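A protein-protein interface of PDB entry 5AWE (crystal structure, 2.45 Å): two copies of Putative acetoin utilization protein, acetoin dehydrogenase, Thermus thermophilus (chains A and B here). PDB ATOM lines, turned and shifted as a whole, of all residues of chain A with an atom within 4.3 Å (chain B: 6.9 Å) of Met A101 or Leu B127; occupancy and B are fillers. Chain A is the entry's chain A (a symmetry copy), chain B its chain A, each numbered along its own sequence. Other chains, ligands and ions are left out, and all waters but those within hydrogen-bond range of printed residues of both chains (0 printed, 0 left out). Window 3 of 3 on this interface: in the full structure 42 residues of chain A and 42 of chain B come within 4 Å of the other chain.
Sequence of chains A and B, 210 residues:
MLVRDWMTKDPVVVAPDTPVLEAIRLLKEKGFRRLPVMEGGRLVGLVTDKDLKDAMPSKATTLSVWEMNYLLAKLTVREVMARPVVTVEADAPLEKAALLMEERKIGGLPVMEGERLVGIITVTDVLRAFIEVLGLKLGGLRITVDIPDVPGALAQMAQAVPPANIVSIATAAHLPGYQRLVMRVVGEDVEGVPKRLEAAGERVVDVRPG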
ATOM      1  N   ALA A  97     -20.703 -33.860  -4.396  1.00  0.00           N
ATOM      2  CA  ALA A  97     -19.659 -33.259  -5.205  1.00  0.00           C
ATOM      3  C   ALA A  97     -19.641 -31.756  -4.967  1.00  0.00           C
ATOM      4  O   ALA A  97     -18.578 -31.173  -4.740  1.00  0.00           O
ATOM      5  CB  ALA A  97     -19.892 -33.564  -6.690  1.00  0.00           C
ATOM      6  N   ALA A  98     -20.815 -31.131  -5.012  1.00  0.00           N
ATOM      7  CA  ALA A  98     -20.902 -29.683  -4.844  1.00  0.00           C
ATOM      8  C   ALA A  98     -20.335 -29.286  -3.489  1.00  0.00           C
ATOM      9  O   ALA A  98     -19.663 -28.261  -3.361  1.00  0.00           O
ATOM     10  CB  ALA A  98     -22.360 -29.209  -4.962  1.00  0.00           C
ATOM     11  N   LEU A  99     -20.608 -30.112  -2.484  1.00  0.00           N
ATOM     12  CA  LEU A  99     -20.139 -29.846  -1.136  1.00  0.00           C
ATOM     13  C   LEU A  99     -18.625 -29.893  -1.092  1.00  0.00           C
ATOM     14  O   LEU A  99     -17.990 -28.972  -0.580  1.00  0.00           O
ATOM     15  CB  LEU A  99     -20.728 -30.863  -0.156  1.00  0.00           C
ATOM     16  CG  LEU A  99     -22.164 -30.562   0.299  1.00  0.00           C
ATOM     17  CD1 LEU A  99     -22.708 -31.728   1.100  1.00  0.00           C
ATOM     18  CD2 LEU A  99     -22.180 -29.283   1.135  1.00  0.00           C
ATOM     19  N   LEU A 100     -18.051 -30.957  -1.646  1.00  0.00           N
ATOM     20  CA  LEU A 100     -16.602 -31.091  -1.688  1.00  0.00           C
ATOM     21  C   LEU A 100     -15.955 -29.940  -2.454  1.00  0.00           C
ATOM     22  O   LEU A 100     -14.960 -29.369  -2.001  1.00  0.00           O
ATOM     23  CB  LEU A 100     -16.217 -32.425  -2.324  1.00  0.00           C
ATOM     24  CG  LEU A 100     -16.430 -33.644  -1.426  1.00  0.00           C
ATOM     25  CD1 LEU A 100     -16.619 -34.873  -2.283  1.00  0.00           C
ATOM     26  CD2 LEU A 100     -15.241 -33.816  -0.476  1.00  0.00           C
ATOM     27  N   MET A 101     -16.522 -29.584  -3.605  1.00  0.00           N
ATOM     28  CA  MET A 101     -15.939 -28.528  -4.427  1.00  0.00           C
ATOM     29  C   MET A 101     -15.932 -27.190  -3.694  1.00  0.00           C
ATOM     30  O   MET A 101     -14.956 -26.453  -3.763  1.00  0.00           O
ATOM     31  CB  MET A 101     -16.701 -28.383  -5.753  1.00  0.00           C
ATOM     32  CG  MET A 101     -16.592 -29.598  -6.665  1.00  0.00           C
ATOM     33  SD  MET A 101     -17.225 -29.341  -8.342  1.00  0.00           S
ATOM     34  CE  MET A 101     -18.746 -28.547  -8.033  1.00  0.00           C
ATOM     35  N   GLU A 102     -17.018 -26.884  -2.988  1.00  0.00           N
ATOM     36  CA  GLU A 102     -17.165 -25.576  -2.350  1.00  0.00           C
ATOM     37  C   GLU A 102     -16.342 -25.498  -1.078  1.00  0.00           C
ATOM     38  O   GLU A 102     -15.771 -24.458  -0.759  1.00  0.00           O
ATOM     39  CB  GLU A 102     -18.636 -25.297  -2.019  1.00  0.00           C
ATOM     40  CG  GLU A 102     -18.921 -23.856  -1.587  1.00  0.00           C
ATOM     41  CD  GLU A 102     -18.615 -23.594  -0.113  1.00  0.00           C
ATOM     42  OE1 GLU A 102     -18.514 -24.566   0.665  1.00  0.00           O
ATOM     43  OE2 GLU A 102     -18.478 -22.411   0.268  1.00  0.00           O
ATOM     44  N   GLU A 103     -16.286 -26.606  -0.352  1.00  0.00           N
ATOM     45  CA  GLU A 103     -15.535 -26.654   0.890  1.00  0.00           C
ATOM     46  C   GLU A 103     -14.069 -26.345   0.603  1.00  0.00           C
ATOM     47  O   GLU A 103     -13.450 -25.518   1.277  1.00  0.00           O
ATOM     48  CB  GLU A 103     -15.666 -28.041   1.521  1.00  0.00           C
ATOM     49  CG  GLU A 103     -14.988 -28.184   2.871  1.00  0.00           C
ATOM     50  CD  GLU A 103     -15.307 -29.512   3.545  1.00  0.00           C
ATOM     51  OE1 GLU A 103     -14.882 -30.568   3.024  1.00  0.00           O
ATOM     52  OE2 GLU A 103     -15.983 -29.499   4.595  1.00  0.00           O
ATOM     53  N   ARG A 104     -13.528 -26.997  -0.423  1.00  0.00           N
ATOM     54  CA  ARG A 104     -12.093 -26.995  -0.651  1.00  0.00           C
ATOM     55  C   ARG A 104     -11.664 -26.179  -1.860  1.00  0.00           C
ATOM     56  O   ARG A 104     -10.554 -26.341  -2.356  1.00  0.00           O
ATOM     57  CB  ARG A 104     -11.603 -28.434  -0.778  1.00  0.00           C
ATOM     58  CG  ARG A 104     -12.042 -29.288   0.397  1.00  0.00           C
ATOM     59  CD  ARG A 104     -11.313 -30.610   0.454  1.00  0.00           C
ATOM     60  NE  ARG A 104     -12.099 -31.612   1.168  1.00  0.00           N
ATOM     61  CZ  ARG A 104     -11.580 -32.571   1.929  1.00  0.00           C
ATOM     62  NH1 ARG A 104     -12.378 -33.439   2.537  1.00  0.00           N
ATOM     63  NH2 ARG A 104     -10.263 -32.656   2.085  1.00  0.00           N
ATOM     64  N   LYS A 105     -12.545 -25.301  -2.328  1.00  0.00           N
ATOM     65  CA  LYS A 105     -12.171 -24.278  -3.304  1.00  0.00           C
ATOM     66  C   LYS A 105     -11.913 -24.830  -4.701  1.00  0.00           C
ATOM     67  O   LYS A 105     -11.514 -24.089  -5.600  1.00  0.00           O
ATOM     68  CB  LYS A 105     -10.924 -23.524  -2.829  1.00  0.00           C
ATOM     69  CG  LYS A 105     -11.104 -22.776  -1.513  1.00  0.00           C
ATOM     70  CD  LYS A 105      -9.881 -21.919  -1.190  1.00  0.00           C
ATOM     71  CE  LYS A 105     -10.105 -21.081   0.060  1.00  0.00           C
ATOM     72  NZ  LYS A 105      -9.041 -20.053   0.238  1.00  0.00           N
ATOM     73  N   ILE A 106     -12.149 -26.127  -4.883  1.00  0.00           N
ATOM     74  CA  ILE A 106     -11.788 -26.818  -6.117  1.00  0.00           C
ATOM     75  C   ILE A 106     -12.857 -26.695  -7.205  1.00  0.00           C
ATOM     76  O   ILE A 106     -14.038 -26.515  -6.914  1.00  0.00           O
ATOM     77  CB  ILE A 106     -11.569 -28.306  -5.854  1.00  0.00           C
ATOM     78  CG1 ILE A 106     -10.717 -28.493  -4.600  1.00  0.00           C
ATOM     79  CG2 ILE A 106     -10.881 -28.938  -7.043  1.00  0.00           C
ATOM     80  CD1 ILE A 106     -10.879 -29.852  -3.980  1.00  0.00           C
ATOM     81  N   GLY A 107     -12.437 -26.807  -8.463  1.00  0.00           N
ATOM     82  CA  GLY A 107     -13.382 -26.728  -9.563  1.00  0.00           C
ATOM     83  C   GLY A 107     -13.648 -28.068 -10.224  1.00  0.00           C
ATOM     84  O   GLY A 107     -14.448 -28.164 -11.155  1.00  0.00           O
ATOM     85  N   LEU A 109     -13.211 -32.729  -9.794  1.00  0.00           N
ATOM     86  CA  LEU A 109     -13.213 -33.832  -8.846  1.00  0.00           C
ATOM     87  C   LEU A 109     -13.126 -35.179  -9.557  1.00  0.00           C
ATOM     88  O   LEU A 109     -13.995 -35.529 -10.361  1.00  0.00           O
ATOM     89  CB  LEU A 109     -14.508 -33.783  -8.032  1.00  0.00           C
ATOM     90  CG  LEU A 109     -14.507 -33.734  -6.504  1.00  0.00           C
ATOM     91  CD1 LEU A 109     -13.455 -32.759  -5.991  1.00  0.00           C
ATOM     92  CD2 LEU A 109     -15.908 -33.312  -6.045  1.00  0.00           C
ATOM     93  N   THR A 122     -17.101 -31.708 -12.824  1.00  0.00           N
ATOM     94  CA  THR A 122     -16.637 -30.346 -12.596  1.00  0.00           C
ATOM     95  C   THR A 122     -17.754 -29.455 -12.080  1.00  0.00           C
ATOM     96  O   THR A 122     -18.911 -29.881 -11.978  1.00  0.00           O
ATOM     97  CB  THR A 122     -16.084 -29.718 -13.887  1.00  0.00           C
ATOM     98  OG1 THR A 122     -17.158 -29.503 -14.809  1.00  0.00           O
ATOM     99  CG2 THR A 122     -15.049 -30.647 -14.530  1.00  0.00           C
ATOM    100  N   VAL A 123     -17.396 -28.215 -11.762  1.00  0.00           N
ATOM    101  CA  VAL A 123     -18.355 -27.231 -11.279  1.00  0.00           C
ATOM    102  C   VAL A 123     -19.456 -26.953 -12.292  1.00  0.00           C
ATOM    103  O   VAL A 123     -20.606 -26.762 -11.908  1.00  0.00           O
ATOM    104  CB  VAL A 123     -17.666 -25.894 -10.900  1.00  0.00           C
ATOM    105  CG1 VAL A 123     -16.873 -26.075  -9.620  1.00  0.00           C
ATOM    106  CG2 VAL A 123     -16.734 -25.430 -12.022  1.00  0.00           C
ATOM    107  N   VAL A 126     -22.006 -29.786 -12.156  1.00  0.00           N
ATOM    108  CA  VAL A 126     -22.878 -29.646 -10.999  1.00  0.00           C
ATOM    109  C   VAL A 126     -23.881 -28.532 -11.269  1.00  0.00           C
ATOM    110  O   VAL A 126     -25.038 -28.610 -10.864  1.00  0.00           O
ATOM    111  CB  VAL A 126     -22.063 -29.324  -9.718  1.00  0.00           C
ATOM    112  CG1 VAL A 126     -22.990 -29.107  -8.541  1.00  0.00           C
ATOM    113  CG2 VAL A 126     -21.111 -30.465  -9.407  1.00  0.00           C
ATOM    114  N   TRP B   6     -24.787 -13.020  -2.709  1.00  0.00           N
ATOM    115  CA  TRP B   6     -23.706 -13.981  -2.833  1.00  0.00           C
ATOM    116  C   TRP B   6     -22.470 -13.436  -3.534  1.00  0.00           C
ATOM    117  O   TRP B   6     -21.401 -14.058  -3.488  1.00  0.00           O
ATOM    118  CB  TRP B   6     -24.226 -15.233  -3.536  1.00  0.00           C
ATOM    119  CG  TRP B   6     -25.415 -15.803  -2.820  1.00  0.00           C
ATOM    120  CD1 TRP B   6     -26.733 -15.504  -3.043  1.00  0.00           C
ATOM    121  CD2 TRP B   6     -25.391 -16.706  -1.715  1.00  0.00           C
ATOM    122  NE1 TRP B   6     -27.527 -16.161  -2.139  1.00  0.00           N
ATOM    123  CE2 TRP B   6     -26.729 -16.908  -1.312  1.00  0.00           C
ATOM    124  CE3 TRP B   6     -24.367 -17.367  -1.026  1.00  0.00           C
ATOM    125  CZ2 TRP B   6     -27.073 -17.743  -0.250  1.00  0.00           C
ATOM    126  CZ3 TRP B   6     -24.709 -18.199   0.034  1.00  0.00           C
ATOM    127  CH2 TRP B   6     -26.052 -18.378   0.410  1.00  0.00           C
ATOM    128  N   LEU B  94     -30.540 -15.349  -7.964  1.00  0.00           N
ATOM    129  CA  LEU B  94     -29.289 -16.073  -7.963  1.00  0.00           C
ATOM    130  C   LEU B  94     -29.233 -17.014  -9.175  1.00  0.00           C
ATOM    131  O   LEU B  94     -28.206 -17.080  -9.857  1.00  0.00           O
ATOM    132  CB  LEU B  94     -29.146 -16.844  -6.639  1.00  0.00           C
ATOM    133  CG  LEU B  94     -27.851 -17.606  -6.327  1.00  0.00           C
ATOM    134  CD1 LEU B  94     -27.835 -18.928  -7.081  1.00  0.00           C
ATOM    135  CD2 LEU B  94     -26.628 -16.739  -6.685  1.00  0.00           C
ATOM    136  N   MET B 101     -23.597 -18.658 -16.388  1.00  0.00           N
ATOM    137  CA  MET B 101     -22.294 -19.303 -16.258  1.00  0.00           C
ATOM    138  C   MET B 101     -22.252 -20.629 -17.009  1.00  0.00           C
ATOM    139  O   MET B 101     -21.262 -20.939 -17.662  1.00  0.00           O
ATOM    140  CB  MET B 101     -21.944 -19.537 -14.781  1.00  0.00           C
ATOM    141  CG  MET B 101     -21.750 -18.256 -13.980  1.00  0.00           C
ATOM    142  SD  MET B 101     -21.051 -18.499 -12.327  1.00  0.00           S
ATOM    143  CE  MET B 101     -22.002 -19.831 -11.728  1.00  0.00           C
ATOM    144  N   THR B 122     -19.053 -15.669  -8.624  1.00  0.00           N
ATOM    145  CA  THR B 122     -18.372 -16.782  -9.273  1.00  0.00           C
ATOM    146  C   THR B 122     -19.137 -18.083  -9.098  1.00  0.00           C
ATOM    147  O   THR B 122     -20.156 -18.132  -8.400  1.00  0.00           O
ATOM    148  CB  THR B 122     -16.955 -16.980  -8.706  1.00  0.00           C
ATOM    149  OG1 THR B 122     -17.047 -17.449  -7.356  1.00  0.00           O
ATOM    150  CG2 THR B 122     -16.183 -15.659  -8.726  1.00  0.00           C
ATOM    151  N   VAL B 123     -18.629 -19.135  -9.734  1.00  0.00           N
ATOM    152  CA  VAL B 123     -19.229 -20.458  -9.644  1.00  0.00           C
ATOM    153  C   VAL B 123     -19.259 -20.982  -8.216  1.00  0.00           C
ATOM    154  O   VAL B 123     -20.223 -21.633  -7.823  1.00  0.00           O
ATOM    155  CB  VAL B 123     -18.497 -21.485 -10.546  1.00  0.00           C
ATOM    156  CG1 VAL B 123     -18.810 -21.200 -12.002  1.00  0.00           C
ATOM    157  CG2 VAL B 123     -16.984 -21.417 -10.322  1.00  0.00           C
ATOM    158  N   THR B 124     -18.238 -20.687  -7.421  1.00  0.00           N
ATOM    159  CA  THR B 124     -18.244 -21.196  -6.055  1.00  0.00           C
ATOM    160  C   THR B 124     -19.203 -20.397  -5.174  1.00  0.00           C
ATOM    161  O   THR B 124     -19.667 -20.902  -4.152  1.00  0.00           O
ATOM    162  CB  THR B 124     -16.813 -21.210  -5.412  1.00  0.00           C
ATOM    163  OG1 THR B 124     -16.362 -19.874  -5.167  1.00  0.00           O
ATOM    164  CG2 THR B 124     -15.823 -21.905  -6.343  1.00  0.00           C
ATOM    165  N   ASP B 125     -19.514 -19.163  -5.570  1.00  0.00           N
ATOM    166  CA  ASP B 125     -20.514 -18.374  -4.847  1.00  0.00           C
ATOM    167  C   ASP B 125     -21.891 -18.977  -5.096  1.00  0.00           C
ATOM    168  O   ASP B 125     -22.697 -19.119  -4.172  1.00  0.00           O
ATOM    169  CB  ASP B 125     -20.515 -16.911  -5.312  1.00  0.00           C
ATOM    170  CG  ASP B 125     -19.216 -16.174  -4.975  1.00  0.00           C
ATOM    171  OD1 ASP B 125     -18.682 -16.343  -3.853  1.00  0.00           O
ATOM    172  OD2 ASP B 125     -18.735 -15.418  -5.846  1.00  0.00           O
ATOM    173  N   VAL B 126     -22.151 -19.335  -6.353  1.00  0.00           N
ATOM    174  CA  VAL B 126     -23.422 -19.942  -6.723  1.00  0.00           C
ATOM    175  C   VAL B 126     -23.538 -21.300  -6.042  1.00  0.00           C
ATOM    176  O   VAL B 126     -24.617 -21.708  -5.626  1.00  0.00           O
ATOM    177  CB  VAL B 126     -23.535 -20.111  -8.262  1.00  0.00           C
ATOM    178  CG1 VAL B 126     -24.827 -20.811  -8.624  1.00  0.00           C
ATOM    179  CG2 VAL B 126     -23.491 -18.753  -8.939  1.00  0.00           C
ATOM    180  N   LEU B 127     -22.417 -21.998  -5.907  1.00  0.00           N
ATOM    181  CA  LEU B 127     -22.448 -23.281  -5.220  1.00  0.00           C
ATOM    182  C   LEU B 127     -22.866 -23.081  -3.775  1.00  0.00           C
ATOM    183  O   LEU B 127     -23.767 -23.750  -3.284  1.00  0.00           O
ATOM    184  CB  LEU B 127     -21.079 -23.963  -5.282  1.00  0.00           C
ATOM    185  CG  LEU B 127     -20.763 -24.674  -6.601  1.00  0.00           C
ATOM    186  CD1 LEU B 127     -19.474 -25.470  -6.462  1.00  0.00           C
ATOM    187  CD2 LEU B 127     -21.925 -25.595  -6.975  1.00  0.00           C
ATOM    188  N   ARG B 128     -22.209 -22.148  -3.098  1.00  0.00           N
ATOM    189  CA  ARG B 128     -22.552 -21.836  -1.717  1.00  0.00           C
ATOM    190  C   ARG B 128     -24.064 -21.577  -1.588  1.00  0.00           C
ATOM    191  O   ARG B 128     -24.724 -22.101  -0.688  1.00  0.00           O
ATOM    192  CB  ARG B 128     -21.755 -20.606  -1.254  1.00  0.00           C
ATOM    193  CG  ARG B 128     -21.664 -20.465   0.264  1.00  0.00           C
ATOM    194  CD  ARG B 128     -20.540 -19.516   0.696  1.00  0.00           C
ATOM    195  NE  ARG B 128     -20.837 -18.121   0.376  1.00  0.00           N
ATOM    196  CZ  ARG B 128     -20.341 -17.482  -0.680  1.00  0.00           C
ATOM    197  NH1 ARG B 128     -19.520 -18.120  -1.511  1.00  0.00           N
ATOM    198  NH2 ARG B 128     -20.667 -16.213  -0.913  1.00  0.00           N
ATOM    199  N   ALA B 129     -24.606 -20.785  -2.507  1.00  0.00           N
ATOM    200  CA  ALA B 129     -26.013 -20.404  -2.464  1.00  0.00           C
ATOM    201  C   ALA B 129     -26.930 -21.625  -2.528  1.00  0.00           C
ATOM    202  O   ALA B 129     -27.859 -21.756  -1.728  1.00  0.00           O
ATOM    203  CB  ALA B 129     -26.331 -19.449  -3.620  1.00  0.00           C
ATOM    204  N   PHE B 130     -26.667 -22.519  -3.480  1.00  0.00           N
ATOM    205  CA  PHE B 130     -27.485 -23.716  -3.639  1.00  0.00           C
ATOM    206  C   PHE B 130     -27.328 -24.608  -2.424  1.00  0.00           C
ATOM    207  O   PHE B 130     -28.274 -25.256  -1.993  1.00  0.00           O
ATOM    208  CB  PHE B 130     -27.089 -24.482  -4.905  1.00  0.00           C
ATOM    209  CG  PHE B 130     -27.628 -23.880  -6.178  1.00  0.00           C
ATOM    210  CD1 PHE B 130     -28.952 -23.469  -6.263  1.00  0.00           C
ATOM    211  CD2 PHE B 130     -26.810 -23.727  -7.291  1.00  0.00           C
ATOM    212  CE1 PHE B 130     -29.462 -22.909  -7.444  1.00  0.00           C
ATOM    213  CE2 PHE B 130     -27.305 -23.171  -8.473  1.00  0.00           C
ATOM    214  CZ  PHE B 130     -28.637 -22.762  -8.549  1.00  0.00           C
ATOM    215  N   ILE B 131     -26.130 -24.617  -1.863  1.00  0.00           N
ATOM    216  CA  ILE B 131     -25.857 -25.407  -0.676  1.00  0.00           C
ATOM    217  C   ILE B 131     -26.674 -24.877   0.498  1.00  0.00           C
ATOM    218  O   ILE B 131     -27.167 -25.647   1.324  1.00  0.00           O
ATOM    219  CB  ILE B 131     -24.361 -25.362  -0.331  1.00  0.00           C
ATOM    220  CG1 ILE B 131     -23.567 -26.121  -1.393  1.00  0.00           C
ATOM    221  CG2 ILE B 131     -24.119 -25.941   1.048  1.00  0.00           C
ATOM    222  CD1 ILE B 131     -22.054 -25.919  -1.303  1.00  0.00           C
ATOM    223  N   GLU B 132     -26.832 -23.562   0.563  1.00  0.00           N
ATOM    224  CA  GLU B 132     -27.599 -22.965   1.641  1.00  0.00           C
ATOM    225  C   GLU B 132     -29.111 -23.165   1.458  1.00  0.00           C
ATOM    226  O   GLU B 132     -29.792 -23.667   2.357  1.00  0.00           O
ATOM    227  CB  GLU B 132     -27.284 -21.473   1.736  1.00  0.00           C
ATOM    228  CG  GLU B 132     -28.044 -20.746   2.830  1.00  0.00           C
ATOM    229  CD  GLU B 132     -27.466 -19.371   3.115  1.00  0.00           C
ATOM    230  OE1 GLU B 132     -28.255 -18.428   3.340  1.00  0.00           O
ATOM    231  OE2 GLU B 132     -26.219 -19.233   3.109  1.00  0.00           O
ATOM    232  N   LEU B 136     -28.137 -28.426   2.183  1.00  0.00           N
ATOM    233  CA  LEU B 136     -27.287 -29.597   2.000  1.00  0.00           C
ATOM    234  C   LEU B 136     -26.375 -29.795   3.207  1.00  0.00           C
ATOM    235  O   LEU B 136     -25.696 -30.814   3.331  1.00  0.00           O
ATOM    236  CB  LEU B 136     -26.444 -29.453   0.721  1.00  0.00           C
ATOM    237  CG  LEU B 136     -27.194 -29.105  -0.576  1.00  0.00           C
ATOM    238  CD1 LEU B 136     -26.221 -29.090  -1.745  1.00  0.00           C
ATOM    239  CD2 LEU B 136     -28.315 -30.104  -0.829  1.00  0.00           C
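O of Trp B6 lies within hydrogen-bond range of NH2 of Arg B128 (3.4 Å).
The side-chain hydroxyl (OG1) of Thr B124 sits at hydrogen-bond distance from the side-chain hydroxyl (OG1) of Thr B122 (3.3 Å).
OD1 of Asp B125 is in salt-bridge range of NH1 of Arg B128 (3.1 Å).
The backbone carbonyl oxygen of Ile B131 sits at hydrogen-bond distance from the backbone NH of Leu B136, 3.1 Å away.
The backbone carbonyl oxygen (O) of Met A101 lies within hydrogen-bond range of the backbone NH (N) of Ile A106 (3.0 Å).
The backbone NH of Val A123 sits close to the side-chain sulfur of Met A101 (3.6 Å).
Ile B131 touches Ala A98 (CD1 to O, 3.9 Å).
Leu A99 touches Ile B131.
Leu A99 touches Leu B136.
Leu B127 touches Met A101 (CD1 to CE, 3.5 Å).
Glu A102 touches Thr B124.
Glu A102 touches Arg B128.
Glu A102 touches Ile B131.
Val A126 touches Leu B127 (CG1 to CD2, 3.99 Å).
Printed residues of chain B within 4 Å of Glu A102: Thr B124 (3.98 Å), Arg B128 (3.6 Å) and Ile B131 (3.5 Å).
Lys A105 touches none of the printed residues of chain B.
Of the printed residues of chain B, Val A126 touches Leu B127 (3.99 Å).
Asp B125 touches none of the printed residues of chain A.
Printed residues of chain A within 4 Å of Leu B127: Met A101 (3.5 Å) and Val A126 (3.99 Å).
Printed residues of chain A within 4 Å of Leu B136: Leu A99.
The nearest printed residue of chain A that does not touch Leu B127 is Val A123 (4.1 Å).
Hydrophobic or aromatic side chains of chain B within 4 Å of the printed part of chain A: Leu B127 and Ile B131.
Of the 15 printed residues of chain A, 5 touch a printed residue of chain B.
Hydrophobic or aromatic side chains of chain A that line the printed part of chain B: Leu A99, Met A101 and Val A126.
Among the printed residues, 8 pairs touch across the chains.
Among the printed residues, no Asp or Glu carboxylate lies within 4 Å of a Lys or Arg side-chain nitrogen of the other chain.
Positions printed for both chains: 101, 122, 123 and 126.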
